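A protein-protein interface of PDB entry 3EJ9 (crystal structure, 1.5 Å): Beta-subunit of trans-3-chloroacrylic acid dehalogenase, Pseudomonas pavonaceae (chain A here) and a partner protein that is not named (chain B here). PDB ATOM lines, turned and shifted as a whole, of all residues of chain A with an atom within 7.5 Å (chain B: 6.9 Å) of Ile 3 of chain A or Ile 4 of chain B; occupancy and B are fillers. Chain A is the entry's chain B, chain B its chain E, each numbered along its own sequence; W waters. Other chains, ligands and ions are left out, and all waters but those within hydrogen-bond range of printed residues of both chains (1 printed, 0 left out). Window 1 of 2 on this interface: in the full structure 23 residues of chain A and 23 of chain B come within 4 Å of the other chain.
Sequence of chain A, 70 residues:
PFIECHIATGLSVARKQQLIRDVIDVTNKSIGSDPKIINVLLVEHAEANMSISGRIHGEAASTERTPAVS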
ATOM      1  N   PRO A   1       4.371 -25.523 -25.598  1.00  0.00           N
ATOM      2  CA  PRO A   1       4.222 -24.085 -25.754  1.00  0.00           C
ATOM      3  C   PRO A   1       5.261 -23.451 -26.682  1.00  0.00           C
ATOM      4  O   PRO A   1       6.362 -23.972 -26.830  1.00  0.00           O
ATOM      5  CB  PRO A   1       4.415 -23.569 -24.328  1.00  0.00           C
ATOM      6  CG  PRO A   1       3.956 -24.705 -23.442  1.00  0.00           C
ATOM      7  CD  PRO A   1       3.924 -25.974 -24.266  1.00  0.00           C
ATOM      8  N   PHE A   2       4.882 -22.344 -27.316  1.00  0.00           N
ATOM      9  CA  PHE A   2       5.805 -21.504 -28.070  1.00  0.00           C
ATOM     10  C   PHE A   2       5.878 -20.136 -27.399  1.00  0.00           C
ATOM     11  O   PHE A   2       4.904 -19.397 -27.365  1.00  0.00           O
ATOM     12  CB  PHE A   2       5.351 -21.371 -29.529  1.00  0.00           C
ATOM     13  CG  PHE A   2       6.170 -20.400 -30.337  1.00  0.00           C
ATOM     14  CD1 PHE A   2       7.558 -20.394 -30.245  1.00  0.00           C
ATOM     15  CD2 PHE A   2       5.553 -19.491 -31.191  1.00  0.00           C
ATOM     16  CE1 PHE A   2       8.320 -19.490 -30.984  1.00  0.00           C
ATOM     17  CE2 PHE A   2       6.310 -18.583 -31.939  1.00  0.00           C
ATOM     18  CZ  PHE A   2       7.695 -18.583 -31.833  1.00  0.00           C
ATOM     19  N   ILE A   3       7.050 -19.837 -26.849  1.00  0.00           N
ATOM     20  CA  ILE A   3       7.281 -18.588 -26.130  1.00  0.00           C
ATOM     21  C   ILE A   3       8.187 -17.696 -26.951  1.00  0.00           C
ATOM     22  O   ILE A   3       9.297 -18.082 -27.267  1.00  0.00           O
ATOM     23  CB  ILE A   3       7.880 -18.854 -24.731  1.00  0.00           C
ATOM     24  CG1 ILE A   3       6.909 -19.706 -23.911  1.00  0.00           C
ATOM     25  CG2 ILE A   3       8.162 -17.539 -23.996  1.00  0.00           C
ATOM     26  CD1 ILE A   3       7.560 -20.468 -22.826  1.00  0.00           C
ATOM     27  N   GLU A   4       7.673 -16.521 -27.307  1.00  0.00           N
ATOM     28  CA  GLU A   4       8.439 -15.495 -28.003  1.00  0.00           C
ATOM     29  C   GLU A   4       8.704 -14.348 -27.044  1.00  0.00           C
ATOM     30  O   GLU A   4       7.780 -13.812 -26.430  1.00  0.00           O
ATOM     31  CB  GLU A   4       7.675 -15.007 -29.236  1.00  0.00           C
ATOM     32  CG  GLU A   4       8.514 -14.200 -30.202  1.00  0.00           C
ATOM     33  CD  GLU A   4       7.850 -13.980 -31.554  1.00  0.00           C
ATOM     34  OE1 GLU A   4       8.283 -13.037 -32.255  1.00  0.00           O
ATOM     35  OE2 GLU A   4       6.928 -14.738 -31.926  1.00  0.00           O
ATOM     36  N   CYS A   5       9.972 -13.984 -26.929  1.00  0.00           N
ATOM     37  CA  CYS A   5      10.406 -12.941 -25.987  1.00  0.00           C
ATOM     38  C   CYS A   5      11.064 -11.808 -26.741  1.00  0.00           C
ATOM     39  O   CYS A   5      12.087 -11.995 -27.390  1.00  0.00           O
ATOM     40  CB  CYS A   5      11.436 -13.488 -24.996  1.00  0.00           C
ATOM     41  SG  CYS A   5      10.908 -14.817 -23.926  1.00  0.00           S
ATOM     42  N   HIS A   6      10.460 -10.634 -26.654  1.00  0.00           N
ATOM     43  CA  HIS A   6      10.986  -9.430 -27.288  1.00  0.00           C
ATOM     44  C   HIS A   6      11.637  -8.589 -26.211  1.00  0.00           C
ATOM     45  O   HIS A   6      10.963  -8.095 -25.297  1.00  0.00           O
ATOM     46  CB  HIS A   6       9.853  -8.665 -27.960  1.00  0.00           C
ATOM     47  CG  HIS A   6       9.234  -9.402 -29.103  1.00  0.00           C
ATOM     48  ND1 HIS A   6       8.040 -10.082 -28.995  1.00  0.00           N
ATOM     49  CD2 HIS A   6       9.661  -9.585 -30.372  1.00  0.00           C
ATOM     50  CE1 HIS A   6       7.756 -10.649 -30.154  1.00  0.00           C
ATOM     51  NE2 HIS A   6       8.720 -10.355 -31.008  1.00  0.00           N
ATOM     52  N   ILE A   7      12.954  -8.457 -26.323  1.00  0.00           N
ATOM     53  CA  ILE A   7      13.762  -7.739 -25.344  1.00  0.00           C
ATOM     54  C   ILE A   7      14.646  -6.695 -26.015  1.00  0.00           C
ATOM     55  O   ILE A   7      14.832  -6.701 -27.238  1.00  0.00           O
ATOM     56  CB  ILE A   7      14.636  -8.710 -24.514  1.00  0.00           C
ATOM     57  CG1 ILE A   7      15.642  -9.443 -25.414  1.00  0.00           C
ATOM     58  CG2 ILE A   7      13.757  -9.670 -23.746  1.00  0.00           C
ATOM     59  CD1 ILE A   7      16.774 -10.136 -24.666  1.00  0.00           C
ATOM     60  N   VAL A  23      13.743 -19.811 -19.229  1.00  0.00           N
ATOM     61  CA  VAL A  23      12.372 -19.801 -19.761  1.00  0.00           C
ATOM     62  C   VAL A  23      11.822 -21.228 -19.864  1.00  0.00           C
ATOM     63  O   VAL A  23      10.688 -21.493 -19.464  1.00  0.00           O
ATOM     64  CB  VAL A  23      12.280 -19.067 -21.131  1.00  0.00           C
ATOM     65  CG1 VAL A  23      10.928 -19.331 -21.806  1.00  0.00           C
ATOM     66  CG2 VAL A  23      12.508 -17.578 -20.941  1.00  0.00           C
ATOM     67  N   ILE A  24      12.637 -22.150 -20.370  1.00  0.00           N
ATOM     68  CA  ILE A  24      12.249 -23.557 -20.452  1.00  0.00           C
ATOM     69  C   ILE A  24      11.947 -24.102 -19.061  1.00  0.00           C
ATOM     70  O   ILE A  24      10.910 -24.730 -18.851  1.00  0.00           O
ATOM     71  CB  ILE A  24      13.336 -24.399 -21.153  1.00  0.00           C
ATOM     72  CG1 ILE A  24      13.413 -24.004 -22.629  1.00  0.00           C
ATOM     73  CG2 ILE A  24      13.076 -25.906 -20.993  1.00  0.00           C
ATOM     74  CD1 ILE A  24      14.730 -24.345 -23.287  1.00  0.00           C
ATOM     75  N   VAL A  26      11.151 -22.525 -16.154  1.00  0.00           N
ATOM     76  CA  VAL A  26       9.983 -21.972 -15.446  1.00  0.00           C
ATOM     77  C   VAL A  26       8.665 -22.405 -16.070  1.00  0.00           C
ATOM     78  O   VAL A  26       7.668 -22.557 -15.375  1.00  0.00           O
ATOM     79  CB  VAL A  26      10.016 -20.421 -15.253  1.00  0.00           C
ATOM     80  CG1 VAL A  26      11.116 -20.017 -14.290  1.00  0.00           C
ATOM     81  CG2 VAL A  26      10.072 -19.656 -16.581  1.00  0.00           C
ATOM     82  N   THR A  27       8.668 -22.593 -17.386  1.00  0.00           N
ATOM     83  CA  THR A  27       7.490 -23.105 -18.078  1.00  0.00           C
ATOM     84  C   THR A  27       7.201 -24.528 -17.600  1.00  0.00           C
ATOM     85  O   THR A  27       6.068 -24.860 -17.249  1.00  0.00           O
ATOM     86  CB  THR A  27       7.677 -23.056 -19.600  1.00  0.00           C
ATOM     87  OG1 THR A  27       7.940 -21.706 -19.984  1.00  0.00           O
ATOM     88  CG2 THR A  27       6.433 -23.555 -20.326  1.00  0.00           C
ATOM     89  N   ASN A  28       8.244 -25.350 -17.560  1.00  0.00           N
ATOM     90  CA  ASN A  28       8.135 -26.712 -17.045  1.00  0.00           C
ATOM     91  C   ASN A  28       7.623 -26.735 -15.610  1.00  0.00           C
ATOM     92  O   ASN A  28       6.760 -27.542 -15.266  1.00  0.00           O
ATOM     93  CB  ASN A  28       9.489 -27.424 -17.140  1.00  0.00           C
ATOM     94  CG  ASN A  28       9.484 -28.780 -16.459  1.00  0.00           C
ATOM     95  OD1 ASN A  28       8.838 -29.721 -16.921  1.00  0.00           O
ATOM     96  ND2 ASN A  28      10.202 -28.885 -15.351  1.00  0.00           N
ATOM     97  N   ILE A  31       3.655 -24.897 -15.500  1.00  0.00           N
ATOM     98  CA  ILE A  31       2.547 -25.600 -16.161  1.00  0.00           C
ATOM     99  C   ILE A  31       2.813 -27.085 -16.438  1.00  0.00           C
ATOM    100  O   ILE A  31       1.947 -27.790 -16.959  1.00  0.00           O
ATOM    101  CB  ILE A  31       2.024 -24.861 -17.442  1.00  0.00           C
ATOM    102  CG1 ILE A  31       3.075 -24.843 -18.557  1.00  0.00           C
ATOM    103  CG2 ILE A  31       1.503 -23.452 -17.099  1.00  0.00           C
ATOM    104  CD1 ILE A  31       2.564 -24.254 -19.866  1.00  0.00           C
ATOM    105  N   ILE A  38       8.345 -27.634 -25.501  1.00  0.00           N
ATOM    106  CA  ILE A  38       8.616 -26.207 -25.265  1.00  0.00           C
ATOM    107  C   ILE A  38       9.529 -25.674 -26.359  1.00  0.00           C
ATOM    108  O   ILE A  38      10.535 -26.286 -26.693  1.00  0.00           O
ATOM    109  CB  ILE A  38       9.224 -25.945 -23.858  1.00  0.00           C
ATOM    110  CG1 ILE A  38       8.295 -26.474 -22.767  1.00  0.00           C
ATOM    111  CG2 ILE A  38       9.473 -24.439 -23.635  1.00  0.00           C
ATOM    112  CD1 ILE A  38       8.905 -26.464 -21.365  1.00  0.00           C
ATOM    113  N   ASN A  39       9.136 -24.544 -26.927  1.00  0.00           N
ATOM    114  CA  ASN A  39       9.859 -23.878 -28.003  1.00  0.00           C
ATOM    115  C   ASN A  39      10.012 -22.415 -27.641  1.00  0.00           C
ATOM    116  O   ASN A  39       9.056 -21.791 -27.173  1.00  0.00           O
ATOM    117  CB  ASN A  39       9.075 -24.009 -29.308  1.00  0.00           C
ATOM    118  CG  ASN A  39       8.633 -25.437 -29.578  1.00  0.00           C
ATOM    119  OD1 ASN A  39       7.519 -25.849 -29.213  1.00  0.00           O
ATOM    120  ND2 ASN A  39       9.510 -26.209 -30.189  1.00  0.00           N
ATOM    121  N   VAL A  40      11.214 -21.879 -27.834  1.00  0.00           N
ATOM    122  CA  VAL A  40      11.525 -20.500 -27.415  1.00  0.00           C
ATOM    123  C   VAL A  40      12.218 -19.734 -28.521  1.00  0.00           C
ATOM    124  O   VAL A  40      13.149 -20.239 -29.147  1.00  0.00           O
ATOM    125  CB  VAL A  40      12.409 -20.442 -26.137  1.00  0.00           C
ATOM    126  CG1 VAL A  40      12.603 -18.983 -25.660  1.00  0.00           C
ATOM    127  CG2 VAL A  40      11.798 -21.266 -25.023  1.00  0.00           C
ATOM    128  N   LEU A  41      11.739 -18.515 -28.747  1.00  0.00           N
ATOM    129  CA  LEU A  41      12.365 -17.583 -29.677  1.00  0.00           C
ATOM    130  C   LEU A  41      12.656 -16.266 -28.951  1.00  0.00           C
ATOM    131  O   LEU A  41      11.763 -15.672 -28.365  1.00  0.00           O
ATOM    132  CB  LEU A  41      11.471 -17.352 -30.900  1.00  0.00           C
ATOM    133  CG  LEU A  41      11.910 -16.269 -31.897  1.00  0.00           C
ATOM    134  CD1 LEU A  41      13.214 -16.652 -32.594  1.00  0.00           C
ATOM    135  CD2 LEU A  41      10.819 -15.973 -32.928  1.00  0.00           C
ATOM    136  N   LEU A  42      13.925 -15.862 -28.958  1.00  0.00           N
ATOM    137  CA  LEU A  42      14.351 -14.563 -28.397  1.00  0.00           C
ATOM    138  C   LEU A  42      14.592 -13.588 -29.529  1.00  0.00           C
ATOM    139  O   LEU A  42      15.308 -13.895 -30.469  1.00  0.00           O
ATOM    140  CB  LEU A  42      15.653 -14.683 -27.598  1.00  0.00           C
ATOM    141  CG  LEU A  42      15.787 -15.501 -26.320  1.00  0.00           C
ATOM    142  CD1 LEU A  42      17.119 -15.157 -25.665  1.00  0.00           C
ATOM    143  CD2 LEU A  42      14.651 -15.298 -25.324  1.00  0.00           C
ATOM    144  N   ILE A  52       5.870   0.261 -23.950  1.00  0.00           N
ATOM    145  CA  ILE A  52       5.057  -0.438 -22.958  1.00  0.00           C
ATOM    146  C   ILE A  52       4.222   0.594 -22.240  1.00  0.00           C
ATOM    147  O   ILE A  52       4.751   1.633 -21.820  1.00  0.00           O
ATOM    148  CB  ILE A  52       5.937  -1.165 -21.910  1.00  0.00           C
ATOM    149  CG1 ILE A  52       6.904  -2.144 -22.580  1.00  0.00           C
ATOM    150  CG2 ILE A  52       5.086  -1.884 -20.854  1.00  0.00           C
ATOM    151  CD1 ILE A  52       6.274  -3.436 -23.089  1.00  0.00           C
ATOM    152  N   PRO B   2       9.858  -5.135 -22.152  1.00  0.00           N
ATOM    153  CA  PRO B   2       9.823  -6.391 -22.880  1.00  0.00           C
ATOM    154  C   PRO B   2       8.406  -6.843 -23.133  1.00  0.00           C
ATOM    155  O   PRO B   2       7.506  -6.526 -22.357  1.00  0.00           O
ATOM    156  CB  PRO B   2      10.508  -7.361 -21.913  1.00  0.00           C
ATOM    157  CG  PRO B   2      11.511  -6.515 -21.221  1.00  0.00           C
ATOM    158  CD  PRO B   2      10.978  -5.101 -21.191  1.00  0.00           C
ATOM    159  N   MET B   3       8.220  -7.578 -24.225  1.00  0.00           N
ATOM    160  CA  MET B   3       6.928  -8.182 -24.534  1.00  0.00           C
ATOM    161  C   MET B   3       7.138  -9.670 -24.744  1.00  0.00           C
ATOM    162  O   MET B   3       8.025 -10.092 -25.488  1.00  0.00           O
ATOM    163  CB  MET B   3       6.270  -7.564 -25.772  1.00  0.00           C
ATOM    164  CG  MET B   3       6.017  -6.072 -25.716  1.00  0.00           C
ATOM    165  SD  MET B   3       7.352  -5.230 -26.568  1.00  0.00           S
ATOM    166  CE  MET B   3       6.750  -3.554 -26.620  1.00  0.00           C
ATOM    167  N   ILE B   4       6.311 -10.457 -24.082  1.00  0.00           N
ATOM    168  CA  ILE B   4       6.422 -11.904 -24.115  1.00  0.00           C
ATOM    169  C   ILE B   4       5.086 -12.451 -24.584  1.00  0.00           C
ATOM    170  O   ILE B   4       4.044 -11.994 -24.146  1.00  0.00           O
ATOM    171  CB  ILE B   4       6.719 -12.482 -22.696  1.00  0.00           C
ATOM    172  CG1 ILE B   4       7.831 -11.710 -21.976  1.00  0.00           C
ATOM    173  CG2 ILE B   4       7.031 -13.986 -22.782  1.00  0.00           C
ATOM    174  CD1 ILE B   4       7.866 -11.981 -20.499  1.00  0.00           C
ATOM    175  N   SER B   5       5.127 -13.438 -25.475  1.00  0.00           N
ATOM    176  CA  SER B   5       3.910 -14.183 -25.807  1.00  0.00           C
ATOM    177  C   SER B   5       4.100 -15.675 -25.608  1.00  0.00           C
ATOM    178  O   SER B   5       5.209 -16.194 -25.710  1.00  0.00           O
ATOM    179  CB  SER B   5       3.448 -13.899 -27.227  1.00  0.00           C
ATOM    180  OG  SER B   5       4.421 -14.296 -28.171  1.00  0.00           O
ATOM    181  N   CYS B   6       3.005 -16.362 -25.315  1.00  0.00           N
ATOM    182  CA  CYS B   6       3.027 -17.807 -25.173  1.00  0.00           C
ATOM    183  C   CYS B   6       1.833 -18.394 -25.897  1.00  0.00           C
ATOM    184  O   CYS B   6       0.696 -18.176 -25.474  1.00  0.00           O
ATOM    185  CB  CYS B   6       2.987 -18.208 -23.697  1.00  0.00           C
ATOM    186  SG  CYS B   6       2.897 -19.988 -23.417  1.00  0.00           S
ATOM    187  N   ASP B   7       2.093 -19.124 -26.978  1.00  0.00           N
ATOM    188  CA  ASP B   7       1.047 -19.876 -27.677  1.00  0.00           C
ATOM    189  C   ASP B   7       0.996 -21.282 -27.097  1.00  0.00           C
ATOM    190  O   ASP B   7       2.004 -21.979 -27.063  1.00  0.00           O
ATOM    191  CB  ASP B   7       1.349 -19.970 -29.181  1.00  0.00           C
ATOM    192  CG  ASP B   7       1.056 -18.682 -29.938  1.00  0.00           C
ATOM    193  OD1 ASP B   7       0.017 -18.609 -30.621  1.00  0.00           O
ATOM    194  OD2 ASP B   7       1.867 -17.740 -29.877  1.00  0.00           O
ATOM    195  N   LEU B  20       2.625 -19.184 -14.516  1.00  0.00           N
ATOM    196  CA  LEU B  20       3.409 -19.001 -15.718  1.00  0.00           C
ATOM    197  C   LEU B  20       3.834 -17.548 -15.856  1.00  0.00           C
ATOM    198  O   LEU B  20       5.006 -17.272 -16.075  1.00  0.00           O
ATOM    199  CB  LEU B  20       2.620 -19.466 -16.947  1.00  0.00           C
ATOM    200  CG  LEU B  20       3.337 -19.346 -18.290  1.00  0.00           C
ATOM    201  CD1 LEU B  20       4.581 -20.225 -18.313  1.00  0.00           C
ATOM    202  CD2 LEU B  20       2.377 -19.727 -19.402  1.00  0.00           C
ATOM    203  N   SER B  21       2.888 -16.618 -15.727  1.00  0.00           N
ATOM    204  CA  SER B  21       3.213 -15.200 -15.891  1.00  0.00           C
ATOM    205  C   SER B  21       4.207 -14.755 -14.816  1.00  0.00           C
ATOM    206  O   SER B  21       5.186 -14.084 -15.117  1.00  0.00           O
ATOM    207  CB  SER B  21       1.954 -14.326 -15.867  1.00  0.00           C
ATOM    208  OG  SER B  21       1.499 -14.100 -14.555  1.00  0.00           O
ATOM    209  N   LEU B  24       7.743 -16.248 -15.741  1.00  0.00           N
ATOM    210  CA  LEU B  24       8.330 -15.599 -16.926  1.00  0.00           C
ATOM    211  C   LEU B  24       8.740 -14.155 -16.649  1.00  0.00           C
ATOM    212  O   LEU B  24       9.812 -13.718 -17.065  1.00  0.00           O
ATOM    213  CB  LEU B  24       7.399 -15.677 -18.144  1.00  0.00           C
ATOM    214  CG  LEU B  24       7.164 -17.081 -18.711  1.00  0.00           C
ATOM    215  CD1 LEU B  24       6.069 -17.045 -19.762  1.00  0.00           C
ATOM    216  CD2 LEU B  24       8.447 -17.691 -19.284  1.00  0.00           C
ATOM    217  N   LEU B  25       7.890 -13.418 -15.943  1.00  0.00           N
ATOM    218  CA  LEU B  25       8.225 -12.051 -15.557  1.00  0.00           C
ATOM    219  C   LEU B  25       9.494 -11.991 -14.712  1.00  0.00           C
ATOM    220  O   LEU B  25      10.356 -11.156 -14.953  1.00  0.00           O
ATOM    221  CB  LEU B  25       7.055 -11.384 -14.834  1.00  0.00           C
ATOM    222  CG  LEU B  25       6.108 -10.526 -15.683  1.00  0.00           C
ATOM    223  CD1 LEU B  25       5.541 -11.266 -16.896  1.00  0.00           C
ATOM    224  CD2 LEU B  25       4.983 -10.044 -14.814  1.00  0.00           C
ATOM    225  N   ILE B  28      12.634 -12.832 -16.940  1.00  0.00           N
ATOM    226  CA  ILE B  28      12.909 -11.717 -17.838  1.00  0.00           C
ATOM    227  C   ILE B  28      13.469 -10.520 -17.076  1.00  0.00           C
ATOM    228  O   ILE B  28      14.446  -9.912 -17.520  1.00  0.00           O
ATOM    229  CB  ILE B  28      11.654 -11.315 -18.651  1.00  0.00           C
ATOM    230  CG1 ILE B  28      11.294 -12.413 -19.664  1.00  0.00           C
ATOM    231  CG2 ILE B  28      11.859  -9.958 -19.353  1.00  0.00           C
ATOM    232  CD1 ILE B  28      12.340 -12.688 -20.732  1.00  0.00           C
ATOM    233  N   ILE B  39       7.021  -4.771 -18.362  1.00  0.00           N
ATOM    234  CA  ILE B  39       6.882  -6.067 -19.022  1.00  0.00           C
ATOM    235  C   ILE B  39       5.415  -6.322 -19.361  1.00  0.00           C
ATOM    236  O   ILE B  39       4.535  -6.083 -18.539  1.00  0.00           O
ATOM    237  CB  ILE B  39       7.469  -7.221 -18.144  1.00  0.00           C
ATOM    238  CG1 ILE B  39       8.952  -6.979 -17.843  1.00  0.00           C
ATOM    239  CG2 ILE B  39       7.290  -8.585 -18.805  1.00  0.00           C
ATOM    240  CD1 ILE B  39       9.520  -7.863 -16.735  1.00  0.00           C
ATOM    241  N   PHE B  40       5.168  -6.778 -20.592  1.00  0.00           N
ATOM    242  CA  PHE B  40       3.838  -7.183 -21.044  1.00  0.00           C
ATOM    243  C   PHE B  40       3.883  -8.661 -21.437  1.00  0.00           C
ATOM    244  O   PHE B  40       4.848  -9.101 -22.064  1.00  0.00           O
ATOM    245  CB  PHE B  40       3.378  -6.330 -22.240  1.00  0.00           C
ATOM    246  CG  PHE B  40       2.149  -6.857 -22.900  1.00  0.00           C
ATOM    247  CD1 PHE B  40       0.891  -6.605 -22.353  1.00  0.00           C
ATOM    248  CD2 PHE B  40       2.244  -7.649 -24.046  1.00  0.00           C
ATOM    249  CE1 PHE B  40      -0.258  -7.113 -22.946  1.00  0.00           C
ATOM    250  CE2 PHE B  40       1.096  -8.160 -24.641  1.00  0.00           C
ATOM    251  CZ  PHE B  40      -0.151  -7.894 -24.092  1.00  0.00           C
ATOM    252  N   PHE B  41       2.827  -9.401 -21.112  1.00  0.00           N
ATOM    253  CA  PHE B  41       2.725 -10.826 -21.444  1.00  0.00           C
ATOM    254  C   PHE B  41       1.324 -11.171 -21.950  1.00  0.00           C
ATOM    255  O   PHE B  41       0.317 -10.738 -21.381  1.00  0.00           O
ATOM    256  CB  PHE B  41       3.081 -11.650 -20.193  1.00  0.00           C
ATOM    257  CG  PHE B  41       2.922 -13.153 -20.348  1.00  0.00           C
ATOM    258  CD1 PHE B  41       3.527 -13.849 -21.389  1.00  0.00           C
ATOM    259  CD2 PHE B  41       2.186 -13.869 -19.417  1.00  0.00           C
ATOM    260  CE1 PHE B  41       3.378 -15.242 -21.507  1.00  0.00           C
ATOM    261  CE2 PHE B  41       2.043 -15.249 -19.516  1.00  0.00           C
ATOM    262  CZ  PHE B  41       2.642 -15.939 -20.551  1.00  0.00           C
ATOM    263  N   VAL B  42       1.294 -11.955 -23.032  1.00  0.00           N
ATOM    264  CA  VAL B  42       0.028 -12.450 -23.580  1.00  0.00           C
ATOM    265  C   VAL B  42       0.111 -13.956 -23.865  1.00  0.00           C
ATOM    266  O   VAL B  42       1.076 -14.448 -24.444  1.00  0.00           O
ATOM    267  CB  VAL B  42      -0.430 -11.643 -24.843  1.00  0.00           C
ATOM    268  CG1 VAL B  42       0.591 -11.725 -25.977  1.00  0.00           C
ATOM    269  CG2 VAL B  42      -1.797 -12.120 -25.325  1.00  0.00           C
ATOM    270  N   ILE B  43      -0.922 -14.670 -23.420  1.00  0.00           N
ATOM    271  CA  ILE B  43      -1.129 -16.082 -23.713  1.00  0.00           C
ATOM    272  C   ILE B  43      -2.119 -16.159 -24.874  1.00  0.00           C
ATOM    273  O   ILE B  43      -3.159 -15.508 -24.842  1.00  0.00           O
ATOM    274  CB  ILE B  43      -1.709 -16.808 -22.490  1.00  0.00           C
ATOM    275  CG1 ILE B  43      -0.681 -16.847 -21.356  1.00  0.00           C
ATOM    276  CG2 ILE B  43      -2.158 -18.218 -22.856  1.00  0.00           C
ATOM    277  CD1 ILE B  43      -1.274 -17.241 -20.016  1.00  0.00           C
ATOM    278  N   ARG B  44      -1.768 -16.936 -25.899  1.00  0.00           N
ATOM    279  CA  ARG B  44      -2.657 -17.189 -27.040  1.00  0.00           C
ATOM    280  C   ARG B  44      -3.027 -18.655 -27.042  1.00  0.00           C
ATOM    281  O   ARG B  44      -2.154 -19.507 -27.144  1.00  0.00           O
ATOM    282  CB  ARG B  44      -1.971 -16.829 -28.357  1.00  0.00           C
ATOM    283  CG  ARG B  44      -1.494 -15.407 -28.441  1.00  0.00           C
ATOM    284  CD  ARG B  44      -1.014 -15.114 -29.843  1.00  0.00           C
ATOM    285  NE  ARG B  44      -0.410 -13.798 -29.931  1.00  0.00           N
ATOM    286  CZ  ARG B  44       0.884 -13.575 -30.125  1.00  0.00           C
ATOM    287  NH1 ARG B  44       1.723 -14.602 -30.266  1.00  0.00           N
ATOM    288  NH2 ARG B  44       1.340 -12.330 -30.205  1.00  0.00           N
HETATM  289  O   HOH W   1       4.152 -16.932 -28.756  1.00  0.00           O
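The backbone carbonyl oxygen (O) of Met 3 of chain B sits at hydrogen-bond distance from the backbone NH (N) of His 6 of chain A (2.8 Å). The backbone NH (N) of Ser 5 of chain B is in hydrogen-bond range of the backbone carbonyl oxygen (O) of Glu 4 of chain A, 2.8 Å away. O of Phe 2 of chain A sits at hydrogen-bond distance from N of Asp 7 of chain B.
The backbone NH of Ile 4 of chain B is in hydrogen-bond range of the backbone carbonyl oxygen of Phe 40 of chain B (2.8 Å). The side-chain hydroxyl of Thr 27 of chain A is in hydrogen-bond range of the backbone carbonyl oxygen of Val 23 of chain A (2.8 Å). The backbone carbonyl oxygen (O) of Cys 6 of chain B sits at hydrogen-bond distance from the backbone NH (N) of Arg 44 of chain B (2.8 Å). A ring nitrogen (NE2) of His 6 of chain A lies within hydrogen-bond range of the side-chain carboxylate of Glu 4 of chain A. The guanidinium group (NH1) of Arg 44 of chain B lies within salt-bridge range of the side-chain carboxylate (OD2) of Asp 7 of chain B (3.2 Å). The backbone carbonyl oxygen (O) of Pro 2 of chain B is in hydrogen-bond range of the backbone NH (N) of Phe 40 of chain B (2.9 Å).
Among the printed residues, merely in contact across the chains: Pro 1 of chain A with Cys 6 of chain B (3.99 Å), Pro 1 of chain A with Asp 7 of chain B (3.3 Å), Phe 2 of chain A with Ser 5 of chain B (3.6 Å), Phe 2 of chain A with Cys 6 of chain B (3.3 Å), Ile 3 of chain A with Ile 4 of chain B (3.9 Å), Ile 3 of chain A with Ser 5 of chain B (3.2 Å), Glu 4 of chain A with Met 3 of chain B (3.8 Å), Glu 4 of chain A with Ile 4 of chain B (3.3 Å), Cys 5 of chain A with Met 3 of chain B (3.7 Å), His 6 of chain A with Pro 2 of chain B (3.2 Å), Val 23 of chain A with Leu 24 of chain B (3.9 Å), Val 26 of chain A with Leu 24 of chain B (3.7 Å), Ile 52 of chain A with Pro 2 of chain B (3.4 Å) and Ile 52 of chain A with Met 3 of chain B (3.6 Å).
Ile 3 of chain A touches just these residues of chain B: Ile 4 and Ser 5. Of the printed residues of chain B, His 6 of chain A touches Pro 2 and Met 3. Ile 31 of chain A touches none of the printed residues of chain B. Printed residues of chain B within 4 Å of Ile 52 of chain A: Pro 2 (3.4 Å) and Met 3 (3.6 Å). Of the printed residues of chain A, Met 3 of chain B touches Glu 4 (3.8 Å), Cys 5 (3.7 Å), His 6 (2.8 Å) and Ile 52 (3.6 Å). Printed residues of chain A within 4 Å of Ile 4 of chain B: Ile 3 (3.9 Å) and Glu 4 (3.3 Å). Printed residues of chain A within 4 Å of Leu 24 of chain B: Val 23 and Val 26. Leu 25 of chain B touches none of the printed residues of chain A. The nearest residue of chain B that does not touch Ile 3 of chain A is Cys 6 of chain B (4.1 Å). The nearest printed residue of chain A that does not touch Ile 4 of chain B is Cys 5 of chain A (4.1 Å). The nearest printed residue of chain B that does not touch His 6 of chain A is Ile 4 of chain B (4.9 Å).
Of the 17 printed residues of chain B, 7 touch a printed residue of chain A. Hydrophobic or aromatic side chains of chain B within 4 Å of the printed part of chain A: Pro 2, Met 3, Ile 4 and Leu 24. Printed residues of chain A that touch a printed residue of chain B: Pro 1, Phe 2, Ile 3, Glu 4, Cys 5, His 6, Val 23, Val 26 and Ile 52.
Water W1 lies within hydrogen-bond range of OD2 of Asp 7 of chain B (2.7 Å), OG of Ser 5 of chain B (2.7 Å) and O of Phe 2 of chain A (2.9 Å).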
